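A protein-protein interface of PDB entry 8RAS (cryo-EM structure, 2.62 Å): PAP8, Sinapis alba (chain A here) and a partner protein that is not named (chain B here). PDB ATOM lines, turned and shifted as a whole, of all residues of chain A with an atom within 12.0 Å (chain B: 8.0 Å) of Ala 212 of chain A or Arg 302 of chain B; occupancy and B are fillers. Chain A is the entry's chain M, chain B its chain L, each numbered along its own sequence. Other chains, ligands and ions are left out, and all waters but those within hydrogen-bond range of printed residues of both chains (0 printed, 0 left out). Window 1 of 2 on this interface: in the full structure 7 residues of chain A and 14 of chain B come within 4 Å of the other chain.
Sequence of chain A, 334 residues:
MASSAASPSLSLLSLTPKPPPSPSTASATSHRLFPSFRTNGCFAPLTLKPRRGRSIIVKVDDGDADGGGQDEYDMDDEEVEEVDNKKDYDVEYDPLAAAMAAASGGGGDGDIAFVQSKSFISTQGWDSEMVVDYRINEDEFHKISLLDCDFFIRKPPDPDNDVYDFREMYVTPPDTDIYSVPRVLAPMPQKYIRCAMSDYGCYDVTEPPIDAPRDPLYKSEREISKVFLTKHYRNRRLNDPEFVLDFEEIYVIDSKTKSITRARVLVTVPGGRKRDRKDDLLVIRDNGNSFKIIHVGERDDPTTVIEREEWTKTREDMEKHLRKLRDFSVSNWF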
ATOM      1  N   PRO A 208      -2.851 -14.352   9.050  1.00  0.00           N
ATOM      2  CA  PRO A 208      -2.879 -15.013   7.750  1.00  0.00           C
ATOM      3  C   PRO A 208      -1.718 -15.978   7.610  1.00  0.00           C
ATOM      4  O   PRO A 208      -0.656 -15.789   8.229  1.00  0.00           O
ATOM      5  CB  PRO A 208      -2.762 -13.844   6.755  1.00  0.00           C
ATOM      6  CG  PRO A 208      -3.000 -12.603   7.553  1.00  0.00           C
ATOM      7  CD  PRO A 208      -2.563 -12.916   8.939  1.00  0.00           C
ATOM      8  N   PRO A 209      -1.875 -17.035   6.816  1.00  0.00           N
ATOM      9  CA  PRO A 209      -0.761 -17.964   6.599  1.00  0.00           C
ATOM     10  C   PRO A 209       0.399 -17.283   5.888  1.00  0.00           C
ATOM     11  O   PRO A 209       0.213 -16.388   5.063  1.00  0.00           O
ATOM     12  CB  PRO A 209      -1.380 -19.068   5.737  1.00  0.00           C
ATOM     13  CG  PRO A 209      -2.561 -18.428   5.086  1.00  0.00           C
ATOM     14  CD  PRO A 209      -3.081 -17.426   6.069  1.00  0.00           C
ATOM     15  N   ILE A 210       1.607 -17.722   6.222  1.00  0.00           N
ATOM     16  CA  ILE A 210       2.839 -17.118   5.728  1.00  0.00           C
ATOM     17  C   ILE A 210       3.310 -17.948   4.538  1.00  0.00           C
ATOM     18  O   ILE A 210       3.836 -19.052   4.704  1.00  0.00           O
ATOM     19  CB  ILE A 210       3.904 -17.046   6.825  1.00  0.00           C
ATOM     20  CG1 ILE A 210       3.412 -16.165   7.974  1.00  0.00           C
ATOM     21  CG2 ILE A 210       5.220 -16.530   6.261  1.00  0.00           C
ATOM     22  CD1 ILE A 210       4.135 -16.395   9.272  1.00  0.00           C
ATOM     23  N   ASP A 211       3.116 -17.422   3.327  1.00  0.00           N
ATOM     24  CA  ASP A 211       3.575 -18.075   2.104  1.00  0.00           C
ATOM     25  C   ASP A 211       4.922 -17.541   1.635  1.00  0.00           C
ATOM     26  O   ASP A 211       5.911 -18.279   1.591  1.00  0.00           O
ATOM     27  CB  ASP A 211       2.531 -17.902   0.992  1.00  0.00           C
ATOM     28  CG  ASP A 211       1.555 -19.048   0.936  1.00  0.00           C
ATOM     29  OD1 ASP A 211       1.583 -19.867   1.870  1.00  0.00           O
ATOM     30  OD2 ASP A 211       0.768 -19.131  -0.031  1.00  0.00           O
ATOM     31  N   ALA A 212       4.979 -16.271   1.295  1.00  0.00           N
ATOM     32  CA  ALA A 212       6.182 -15.661   0.763  1.00  0.00           C
ATOM     33  C   ALA A 212       7.083 -15.195   1.894  1.00  0.00           C
ATOM     34  O   ALA A 212       6.640 -15.064   3.039  1.00  0.00           O
ATOM     35  CB  ALA A 212       5.816 -14.485  -0.139  1.00  0.00           C
ATOM     36  N   PRO A 213       8.365 -14.963   1.616  1.00  0.00           N
ATOM     37  CA  PRO A 213       9.227 -14.354   2.634  1.00  0.00           C
ATOM     38  C   PRO A 213       8.681 -13.000   3.059  1.00  0.00           C
ATOM     39  O   PRO A 213       8.150 -12.242   2.245  1.00  0.00           O
ATOM     40  CB  PRO A 213      10.578 -14.221   1.923  1.00  0.00           C
ATOM     41  CG  PRO A 213      10.556 -15.271   0.878  1.00  0.00           C
ATOM     42  CD  PRO A 213       9.130 -15.416   0.440  1.00  0.00           C
ATOM     43  N   ARG A 214       8.805 -12.715   4.356  1.00  0.00           N
ATOM     44  CA  ARG A 214       8.355 -11.453   4.947  1.00  0.00           C
ATOM     45  C   ARG A 214       6.845 -11.261   4.816  1.00  0.00           C
ATOM     46  O   ARG A 214       6.364 -10.131   4.717  1.00  0.00           O
ATOM     47  CB  ARG A 214       9.093 -10.259   4.335  1.00  0.00           C
ATOM     48  CG  ARG A 214      10.601 -10.366   4.396  1.00  0.00           C
ATOM     49  CD  ARG A 214      11.256  -9.341   3.493  1.00  0.00           C
ATOM     50  NE  ARG A 214      10.969  -9.586   2.086  1.00  0.00           N
ATOM     51  CZ  ARG A 214      11.664 -10.406   1.309  1.00  0.00           C
ATOM     52  NH1 ARG A 214      12.700 -11.085   1.772  1.00  0.00           N
ATOM     53  NH2 ARG A 214      11.310 -10.549   0.035  1.00  0.00           N
ATOM     54  N   ASP A 215       6.086 -12.351   4.812  1.00  0.00           N
ATOM     55  CA  ASP A 215       4.636 -12.228   4.833  1.00  0.00           C
ATOM     56  C   ASP A 215       4.188 -11.677   6.185  1.00  0.00           C
ATOM     57  O   ASP A 215       4.794 -11.992   7.213  1.00  0.00           O
ATOM     58  CB  ASP A 215       3.970 -13.577   4.569  1.00  0.00           C
ATOM     59  CG  ASP A 215       3.390 -13.676   3.173  1.00  0.00           C
ATOM     60  OD1 ASP A 215       3.204 -12.621   2.530  1.00  0.00           O
ATOM     61  OD2 ASP A 215       3.114 -14.805   2.720  1.00  0.00           O
ATOM     62  N   PRO A 216       3.143 -10.850   6.217  1.00  0.00           N
ATOM     63  CA  PRO A 216       2.741 -10.225   7.483  1.00  0.00           C
ATOM     64  C   PRO A 216       2.334 -11.260   8.521  1.00  0.00           C
ATOM     65  O   PRO A 216       1.674 -12.254   8.212  1.00  0.00           O
ATOM     66  CB  PRO A 216       1.559  -9.336   7.079  1.00  0.00           C
ATOM     67  CG  PRO A 216       1.059  -9.920   5.805  1.00  0.00           C
ATOM     68  CD  PRO A 216       2.267 -10.454   5.103  1.00  0.00           C
ATOM     69  N   LEU A 217       2.736 -11.012   9.768  1.00  0.00           N
ATOM     70  CA  LEU A 217       2.384 -11.900  10.866  1.00  0.00           C
ATOM     71  C   LEU A 217       0.937 -11.741  11.303  1.00  0.00           C
ATOM     72  O   LEU A 217       0.372 -12.672  11.885  1.00  0.00           O
ATOM     73  CB  LEU A 217       3.312 -11.656  12.058  1.00  0.00           C
ATOM     74  CG  LEU A 217       4.605 -12.473  12.090  1.00  0.00           C
ATOM     75  CD1 LEU A 217       5.546 -11.932  13.151  1.00  0.00           C
ATOM     76  CD2 LEU A 217       4.308 -13.939  12.332  1.00  0.00           C
ATOM     77  N   TYR A 218       0.329 -10.588  11.035  1.00  0.00           N
ATOM     78  CA  TYR A 218      -1.061 -10.347  11.384  1.00  0.00           C
ATOM     79  C   TYR A 218      -1.669  -9.422  10.343  1.00  0.00           C
ATOM     80  O   TYR A 218      -0.961  -8.746   9.594  1.00  0.00           O
ATOM     81  CB  TYR A 218      -1.196  -9.750  12.791  1.00  0.00           C
ATOM     82  CG  TYR A 218      -0.753  -8.307  12.896  1.00  0.00           C
ATOM     83  CD1 TYR A 218       0.576  -7.983  13.135  1.00  0.00           C
ATOM     84  CD2 TYR A 218      -1.665  -7.268  12.765  1.00  0.00           C
ATOM     85  CE1 TYR A 218       0.984  -6.668  13.231  1.00  0.00           C
ATOM     86  CE2 TYR A 218      -1.266  -5.950  12.858  1.00  0.00           C
ATOM     87  CZ  TYR A 218       0.059  -5.656  13.094  1.00  0.00           C
ATOM     88  OH  TYR A 218       0.460  -4.345  13.190  1.00  0.00           O
ATOM     89  N   GLU B 121      18.907  -3.474  -1.628  1.00  0.00           N
ATOM     90  CA  GLU B 121      18.109  -4.694  -1.585  1.00  0.00           C
ATOM     91  C   GLU B 121      16.641  -4.307  -1.640  1.00  0.00           C
ATOM     92  O   GLU B 121      16.142  -3.640  -0.729  1.00  0.00           O
ATOM     93  CB  GLU B 121      18.402  -5.505  -0.321  1.00  0.00           C
ATOM     94  CG  GLU B 121      19.764  -6.170  -0.313  1.00  0.00           C
ATOM     95  CD  GLU B 121      20.048  -6.895   0.985  1.00  0.00           C
ATOM     96  OE1 GLU B 121      19.416  -6.555   2.007  1.00  0.00           O
ATOM     97  OE2 GLU B 121      20.902  -7.805   0.984  1.00  0.00           O
ATOM     98  N   ILE B 122      15.954  -4.723  -2.694  1.00  0.00           N
ATOM     99  CA  ILE B 122      14.548  -4.398  -2.911  1.00  0.00           C
ATOM    100  C   ILE B 122      13.741  -5.688  -2.796  1.00  0.00           C
ATOM    101  O   ILE B 122      13.951  -6.614  -3.590  1.00  0.00           O
ATOM    102  CB  ILE B 122      14.321  -3.724  -4.274  1.00  0.00           C
ATOM    103  CG1 ILE B 122      15.155  -2.447  -4.382  1.00  0.00           C
ATOM    104  CG2 ILE B 122      12.850  -3.410  -4.471  1.00  0.00           C
ATOM    105  CD1 ILE B 122      16.429  -2.609  -5.180  1.00  0.00           C
ATOM    106  N   PRO B 123      12.831  -5.799  -1.831  1.00  0.00           N
ATOM    107  CA  PRO B 123      12.024  -7.016  -1.714  1.00  0.00           C
ATOM    108  C   PRO B 123      11.091  -7.200  -2.899  1.00  0.00           C
ATOM    109  O   PRO B 123      10.655  -6.240  -3.538  1.00  0.00           O
ATOM    110  CB  PRO B 123      11.235  -6.795  -0.416  1.00  0.00           C
ATOM    111  CG  PRO B 123      12.012  -5.766   0.333  1.00  0.00           C
ATOM    112  CD  PRO B 123      12.596  -4.873  -0.713  1.00  0.00           C
ATOM    113  N   HIS B 124      10.782  -8.467  -3.182  1.00  0.00           N
ATOM    114  CA  HIS B 124       9.947  -8.804  -4.328  1.00  0.00           C
ATOM    115  C   HIS B 124       8.523  -8.282  -4.178  1.00  0.00           C
ATOM    116  O   HIS B 124       7.890  -7.924  -5.177  1.00  0.00           O
ATOM    117  CB  HIS B 124       9.936 -10.319  -4.529  1.00  0.00           C
ATOM    118  CG  HIS B 124       8.958 -10.788  -5.559  1.00  0.00           C
ATOM    119  ND1 HIS B 124       9.060 -10.450  -6.890  1.00  0.00           N
ATOM    120  CD2 HIS B 124       7.863 -11.575  -5.453  1.00  0.00           C
ATOM    121  CE1 HIS B 124       8.068 -11.006  -7.561  1.00  0.00           C
ATOM    122  NE2 HIS B 124       7.326 -11.695  -6.712  1.00  0.00           N
ATOM    123  N   GLU B 125       8.004  -8.227  -2.950  1.00  0.00           N
ATOM    124  CA  GLU B 125       6.613  -7.846  -2.734  1.00  0.00           C
ATOM    125  C   GLU B 125       6.326  -6.391  -3.082  1.00  0.00           C
ATOM    126  O   GLU B 125       5.152  -6.018  -3.170  1.00  0.00           O
ATOM    127  CB  GLU B 125       6.215  -8.112  -1.282  1.00  0.00           C
ATOM    128  CG  GLU B 125       7.078  -7.395  -0.261  1.00  0.00           C
ATOM    129  CD  GLU B 125       8.156  -8.287   0.317  1.00  0.00           C
ATOM    130  OE1 GLU B 125       8.467  -9.323  -0.305  1.00  0.00           O
ATOM    131  OE2 GLU B 125       8.691  -7.953   1.393  1.00  0.00           O
ATOM    132  N   LEU B 126       7.351  -5.566  -3.275  1.00  0.00           N
ATOM    133  CA  LEU B 126       7.171  -4.159  -3.602  1.00  0.00           C
ATOM    134  C   LEU B 126       7.225  -3.887  -5.100  1.00  0.00           C
ATOM    135  O   LEU B 126       7.174  -2.724  -5.509  1.00  0.00           O
ATOM    136  CB  LEU B 126       8.223  -3.314  -2.881  1.00  0.00           C
ATOM    137  CG  LEU B 126       8.213  -3.399  -1.355  1.00  0.00           C
ATOM    138  CD1 LEU B 126       9.199  -2.413  -0.766  1.00  0.00           C
ATOM    139  CD2 LEU B 126       6.817  -3.149  -0.809  1.00  0.00           C
ATOM    140  N   MET B 127       7.323  -4.926  -5.921  1.00  0.00           N
ATOM    141  CA  MET B 127       7.447  -4.780  -7.364  1.00  0.00           C
ATOM    142  C   MET B 127       6.108  -5.025  -8.050  1.00  0.00           C
ATOM    143  O   MET B 127       5.155  -5.534  -7.458  1.00  0.00           O
ATOM    144  CB  MET B 127       8.500  -5.748  -7.910  1.00  0.00           C
ATOM    145  CG  MET B 127       9.859  -5.637  -7.249  1.00  0.00           C
ATOM    146  SD  MET B 127      10.969  -6.948  -7.786  1.00  0.00           S
ATOM    147  CE  MET B 127      12.390  -6.632  -6.747  1.00  0.00           C
ATOM    148  N   PHE B 139       3.313 -11.421 -10.482  1.00  0.00           N
ATOM    149  CA  PHE B 139       4.023 -11.786  -9.258  1.00  0.00           C
ATOM    150  C   PHE B 139       4.464 -10.521  -8.536  1.00  0.00           C
ATOM    151  O   PHE B 139       5.335  -9.792  -9.051  1.00  0.00           O
ATOM    152  CB  PHE B 139       5.227 -12.672  -9.563  1.00  0.00           C
ATOM    153  CG  PHE B 139       4.901 -13.864 -10.409  1.00  0.00           C
ATOM    154  CD1 PHE B 139       4.526 -15.061  -9.826  1.00  0.00           C
ATOM    155  CD2 PHE B 139       4.974 -13.788 -11.789  1.00  0.00           C
ATOM    156  CE1 PHE B 139       4.226 -16.158 -10.604  1.00  0.00           C
ATOM    157  CE2 PHE B 139       4.675 -14.881 -12.571  1.00  0.00           C
ATOM    158  CZ  PHE B 139       4.301 -16.067 -11.978  1.00  0.00           C
ATOM    159  N   PRO B 140       3.910 -10.217  -7.356  1.00  0.00           N
ATOM    160  CA  PRO B 140       2.862 -10.955  -6.635  1.00  0.00           C
ATOM    161  C   PRO B 140       1.492 -10.763  -7.276  1.00  0.00           C
ATOM    162  O   PRO B 140       1.241  -9.754  -7.928  1.00  0.00           O
ATOM    163  CB  PRO B 140       2.934 -10.356  -5.226  1.00  0.00           C
ATOM    164  CG  PRO B 140       3.394  -8.949  -5.453  1.00  0.00           C
ATOM    165  CD  PRO B 140       4.371  -9.042  -6.596  1.00  0.00           C
ATOM    166  N   ARG B 267      13.926 -16.794 -10.627  1.00  0.00           N
ATOM    167  CA  ARG B 267      13.360 -18.024 -10.094  1.00  0.00           C
ATOM    168  C   ARG B 267      12.608 -17.700  -8.810  1.00  0.00           C
ATOM    169  O   ARG B 267      13.178 -17.117  -7.883  1.00  0.00           O
ATOM    170  CB  ARG B 267      14.445 -19.065  -9.827  1.00  0.00           C
ATOM    171  CG  ARG B 267      13.918 -20.312  -9.137  1.00  0.00           C
ATOM    172  CD  ARG B 267      14.996 -21.371  -8.981  1.00  0.00           C
ATOM    173  NE  ARG B 267      15.971 -21.015  -7.958  1.00  0.00           N
ATOM    174  CZ  ARG B 267      15.742 -21.064  -6.652  1.00  0.00           C
ATOM    175  NH1 ARG B 267      14.575 -21.458  -6.170  1.00  0.00           N
ATOM    176  NH2 ARG B 267      16.707 -20.712  -5.810  1.00  0.00           N
ATOM    177  N   ILE B 268      11.333 -18.072  -8.763  1.00  0.00           N
ATOM    178  CA  ILE B 268      10.506 -17.921  -7.573  1.00  0.00           C
ATOM    179  C   ILE B 268      10.095 -19.319  -7.139  1.00  0.00           C
ATOM    180  O   ILE B 268       9.352 -20.005  -7.853  1.00  0.00           O
ATOM    181  CB  ILE B 268       9.280 -17.036  -7.829  1.00  0.00           C
ATOM    182  CG1 ILE B 268       9.717 -15.597  -8.109  1.00  0.00           C
ATOM    183  CG2 ILE B 268       8.334 -17.087  -6.644  1.00  0.00           C
ATOM    184  CD1 ILE B 268       8.619 -14.721  -8.660  1.00  0.00           C
ATOM    185  N   GLY B 269      10.570 -19.743  -5.972  1.00  0.00           N
ATOM    186  CA  GLY B 269      10.343 -21.100  -5.525  1.00  0.00           C
ATOM    187  C   GLY B 269      11.022 -22.106  -6.429  1.00  0.00           C
ATOM    188  O   GLY B 269      12.252 -22.203  -6.449  1.00  0.00           O
ATOM    189  N   ALA B 270      10.228 -22.862  -7.184  1.00  0.00           N
ATOM    190  CA  ALA B 270      10.745 -23.813  -8.156  1.00  0.00           C
ATOM    191  C   ALA B 270      10.466 -23.400  -9.592  1.00  0.00           C
ATOM    192  O   ALA B 270      10.781 -24.159 -10.514  1.00  0.00           O
ATOM    193  CB  ALA B 270      10.160 -25.206  -7.896  1.00  0.00           C
ATOM    194  N   TRP B 297      19.493 -11.155  -8.943  1.00  0.00           N
ATOM    195  CA  TRP B 297      18.282 -11.616  -8.280  1.00  0.00           C
ATOM    196  C   TRP B 297      18.624 -12.711  -7.280  1.00  0.00           C
ATOM    197  O   TRP B 297      19.284 -13.695  -7.627  1.00  0.00           O
ATOM    198  CB  TRP B 297      17.272 -12.130  -9.307  1.00  0.00           C
ATOM    199  CG  TRP B 297      16.126 -12.885  -8.710  1.00  0.00           C
ATOM    200  CD1 TRP B 297      15.976 -14.238  -8.658  1.00  0.00           C
ATOM    201  CD2 TRP B 297      14.963 -12.328  -8.088  1.00  0.00           C
ATOM    202  NE1 TRP B 297      14.795 -14.560  -8.038  1.00  0.00           N
ATOM    203  CE2 TRP B 297      14.153 -13.405  -7.679  1.00  0.00           C
ATOM    204  CE3 TRP B 297      14.528 -11.024  -7.835  1.00  0.00           C
ATOM    205  CZ2 TRP B 297      12.936 -13.218  -7.032  1.00  0.00           C
ATOM    206  CZ3 TRP B 297      13.320 -10.841  -7.193  1.00  0.00           C
ATOM    207  CH2 TRP B 297      12.537 -11.931  -6.799  1.00  0.00           C
ATOM    208  N   ARG B 298      18.175 -12.536  -6.038  1.00  0.00           N
ATOM    209  CA  ARG B 298      18.383 -13.532  -4.999  1.00  0.00           C
ATOM    210  C   ARG B 298      17.095 -14.317  -4.812  1.00  0.00           C
ATOM    211  O   ARG B 298      16.117 -13.765  -4.288  1.00  0.00           O
ATOM    212  CB  ARG B 298      18.800 -12.865  -3.690  1.00  0.00           C
ATOM    213  CG  ARG B 298      19.816 -13.652  -2.885  1.00  0.00           C
ATOM    214  CD  ARG B 298      19.819 -13.224  -1.430  1.00  0.00           C
ATOM    215  NE  ARG B 298      20.405 -11.903  -1.246  1.00  0.00           N
ATOM    216  CZ  ARG B 298      20.031 -11.041  -0.312  1.00  0.00           C
ATOM    217  NH1 ARG B 298      19.064 -11.325   0.545  1.00  0.00           N
ATOM    218  NH2 ARG B 298      20.642  -9.862  -0.234  1.00  0.00           N
ATOM    219  N   PRO B 299      17.039 -15.590  -5.214  1.00  0.00           N
ATOM    220  CA  PRO B 299      15.756 -16.307  -5.195  1.00  0.00           C
ATOM    221  C   PRO B 299      15.359 -16.862  -3.839  1.00  0.00           C
ATOM    222  O   PRO B 299      14.164 -17.099  -3.622  1.00  0.00           O
ATOM    223  CB  PRO B 299      15.972 -17.450  -6.203  1.00  0.00           C
ATOM    224  CG  PRO B 299      17.367 -17.267  -6.761  1.00  0.00           C
ATOM    225  CD  PRO B 299      18.111 -16.397  -5.811  1.00  0.00           C
ATOM    226  N   LYS B 300      16.311 -17.086  -2.928  1.00  0.00           N
ATOM    227  CA  LYS B 300      15.981 -17.746  -1.668  1.00  0.00           C
ATOM    228  C   LYS B 300      15.028 -16.906  -0.826  1.00  0.00           C
ATOM    229  O   LYS B 300      14.076 -17.435  -0.240  1.00  0.00           O
ATOM    230  CB  LYS B 300      17.256 -18.062  -0.890  1.00  0.00           C
ATOM    231  CG  LYS B 300      17.094 -19.194   0.111  1.00  0.00           C
ATOM    232  CD  LYS B 300      18.436 -19.691   0.616  1.00  0.00           C
ATOM    233  CE  LYS B 300      19.052 -20.682  -0.353  1.00  0.00           C
ATOM    234  NZ  LYS B 300      18.376 -22.006  -0.300  1.00  0.00           N
ATOM    235  N   ASP B 301      15.266 -15.598  -0.748  1.00  0.00           N
ATOM    236  CA  ASP B 301      14.384 -14.693  -0.022  1.00  0.00           C
ATOM    237  C   ASP B 301      13.619 -13.758  -0.949  1.00  0.00           C
ATOM    238  O   ASP B 301      12.935 -12.849  -0.466  1.00  0.00           O
ATOM    239  CB  ASP B 301      15.178 -13.881   1.000  1.00  0.00           C
ATOM    240  CG  ASP B 301      16.415 -13.256   0.404  1.00  0.00           C
ATOM    241  OD1 ASP B 301      16.734 -13.572  -0.759  1.00  0.00           O
ATOM    242  OD2 ASP B 301      17.067 -12.447   1.096  1.00  0.00           O
ATOM    243  N   ARG B 302      13.723 -13.956  -2.264  1.00  0.00           N
ATOM    244  CA  ARG B 302      13.028 -13.143  -3.260  1.00  0.00           C
ATOM    245  C   ARG B 302      13.383 -11.663  -3.102  1.00  0.00           C
ATOM    246  O   ARG B 302      12.542 -10.815  -2.805  1.00  0.00           O
ATOM    247  CB  ARG B 302      11.514 -13.366  -3.187  1.00  0.00           C
ATOM    248  CG  ARG B 302      11.105 -14.825  -3.282  1.00  0.00           C
ATOM    249  CD  ARG B 302       9.609 -14.963  -3.478  1.00  0.00           C
ATOM    250  NE  ARG B 302       9.137 -16.305  -3.167  1.00  0.00           N
ATOM    251  CZ  ARG B 302       7.859 -16.660  -3.134  1.00  0.00           C
ATOM    252  NH1 ARG B 302       6.896 -15.791  -3.390  1.00  0.00           N
ATOM    253  NH2 ARG B 302       7.541 -17.915  -2.837  1.00  0.00           N
ATOM    254  N   ILE B 303      14.663 -11.369  -3.302  1.00  0.00           N
ATOM    255  CA  ILE B 303      15.194 -10.018  -3.181  1.00  0.00           C
ATOM    256  C   ILE B 303      16.044  -9.719  -4.406  1.00  0.00           C
ATOM    257  O   ILE B 303      16.829 -10.565  -4.851  1.00  0.00           O
ATOM    258  CB  ILE B 303      16.015  -9.850  -1.882  1.00  0.00           C
ATOM    259  CG1 ILE B 303      15.130  -9.300  -0.764  1.00  0.00           C
ATOM    260  CG2 ILE B 303      17.223  -8.951  -2.099  1.00  0.00           C
ATOM    261  CD1 ILE B 303      15.840  -9.160   0.558  1.00  0.00           C
ATOM    262  N   LEU B 304      15.877  -8.524  -4.964  1.00  0.00           N
ATOM    263  CA  LEU B 304      16.734  -8.051  -6.042  1.00  0.00           C
ATOM    264  C   LEU B 304      17.886  -7.257  -5.445  1.00  0.00           C
ATOM    265  O   LEU B 304      17.665  -6.277  -4.728  1.00  0.00           O
ATOM    266  CB  LEU B 304      15.960  -7.191  -7.036  1.00  0.00           C
ATOM    267  CG  LEU B 304      16.868  -6.549  -8.085  1.00  0.00           C
ATOM    268  CD1 LEU B 304      17.203  -7.550  -9.173  1.00  0.00           C
ATOM    269  CD2 LEU B 304      16.240  -5.301  -8.672  1.00  0.00           C
ATOM    270  N   GLU B 305      19.109  -7.675  -5.746  1.00  0.00           N
ATOM    271  CA  GLU B 305      20.305  -7.027  -5.234  1.00  0.00           C
ATOM    272  C   GLU B 305      20.898  -6.105  -6.287  1.00  0.00           C
ATOM    273  O   GLU B 305      20.979  -6.460  -7.466  1.00  0.00           O
ATOM    274  CB  GLU B 305      21.355  -8.056  -4.818  1.00  0.00           C
ATOM    275  CG  GLU B 305      21.140  -8.660  -3.449  1.00  0.00           C
ATOM    276  CD  GLU B 305      21.888  -9.965  -3.277  1.00  0.00           C
ATOM    277  OE1 GLU B 305      21.881 -10.782  -4.222  1.00  0.00           O
ATOM    278  OE2 GLU B 305      22.484 -10.173  -2.201  1.00  0.00           O
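Printed residues of chain A that touch a printed residue of chain B: Ala 212, Pro 213 and Arg 214. Hydrophobic or aromatic side chains of chain A that line the printed part of chain B: Ala 212 and Pro 213. Printed residues of chain B that touch a printed residue of chain A: Pro 123, His 124, Glu 125, Asp 301, Arg 302 and Ile 303. Among the printed residues, 10 pairs touch across the chains.
The backbone carbonyl oxygen (O) of Ile 303 of chain B is in hydrogen-bond range of the backbone NH (N) of Arg 298 of chain B, 2.7 Å away. The side-chain carboxylate (OD1) of Asp 301 of chain B is in salt-bridge range of the guanidinium group (NH1) of Arg 298 of chain B, at 3.5 Å. The backbone carbonyl oxygen (O) of Arg 302 of chain B lies within hydrogen-bond range of the backbone NH (N) of His 124 of chain B, 3.0 Å away. N of Ala 212 of chain A sits at hydrogen-bond distance from OD2 of Asp 215 of chain A (2.8 Å).
OE2 of Glu 125 of chain B lies within salt-bridge range of NE of Arg 214 of chain A, at 2.9 Å. NH2 of Arg 214 of chain A is in hydrogen-bond range of O of Arg 302 of chain B (3.1 Å). O of Asp 301 of chain B is in hydrogen-bond range of NH1 of Arg 214 of chain A.
Pro 209 of chain A touches none of the printed residues of chain B. Of chain B, only Arg 302 comes within 4 Å of Ala 212 of chain A. Pro 213 of chain A touches just these residues of chain B: Glu 125, Asp 301 and Arg 302. Printed residues of chain B within 4 Å of Arg 214 of chain A: Pro 123 (3.8 Å), His 124 (3.9 Å), Glu 125 (2.9 Å), Asp 301 (2.9 Å), Arg 302 (3.1 Å) and Ile 303 (3.9 Å). Printed residues of chain A within 4 Å of Glu 125 of chain B: Pro 213 (3.9 Å) and Arg 214 (2.9 Å). Leu 126 of chain B touches none of the printed residues of chain A. No residue of chain A comes within 4 Å of Ile 268 of chain B. No residue of chain A comes within 4 Å of Gly 269 of chain B. Pro 299 of chain B touches none of the printed residues of chain A. Of chain A, only Ala 212, Pro 213 and Arg 214 come within 4 Å of Arg 302 of chain B. The nearest residue of chain B that does not touch Ala 212 of chain A is Glu 125 of chain B (5.8 Å). The nearest residue of chain A that does not touch Arg 302 of chain B is Asp 211 of chain A (4.7 Å). The nearest printed residue of chain A that does not touch Glu 125 of chain B is Ala 212 of chain A (5.8 Å).
Arg 302 of chain B touches Ala 212 of chain A. Pro 213 of chain A touches Glu 125 of chain B. Asp 301 of chain B touches Pro 213 of chain A. CD of Pro 213 of chain A touches NE of Arg 302 of chain B (3.7 Å). Arg 214 of chain A touches Pro 123 of chain B. Arg 214 of chain A touches His 124 of chain B. Ile 303 of chain B touches Arg 214 of chain A (CD1 to NH1, 3.9 Å).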
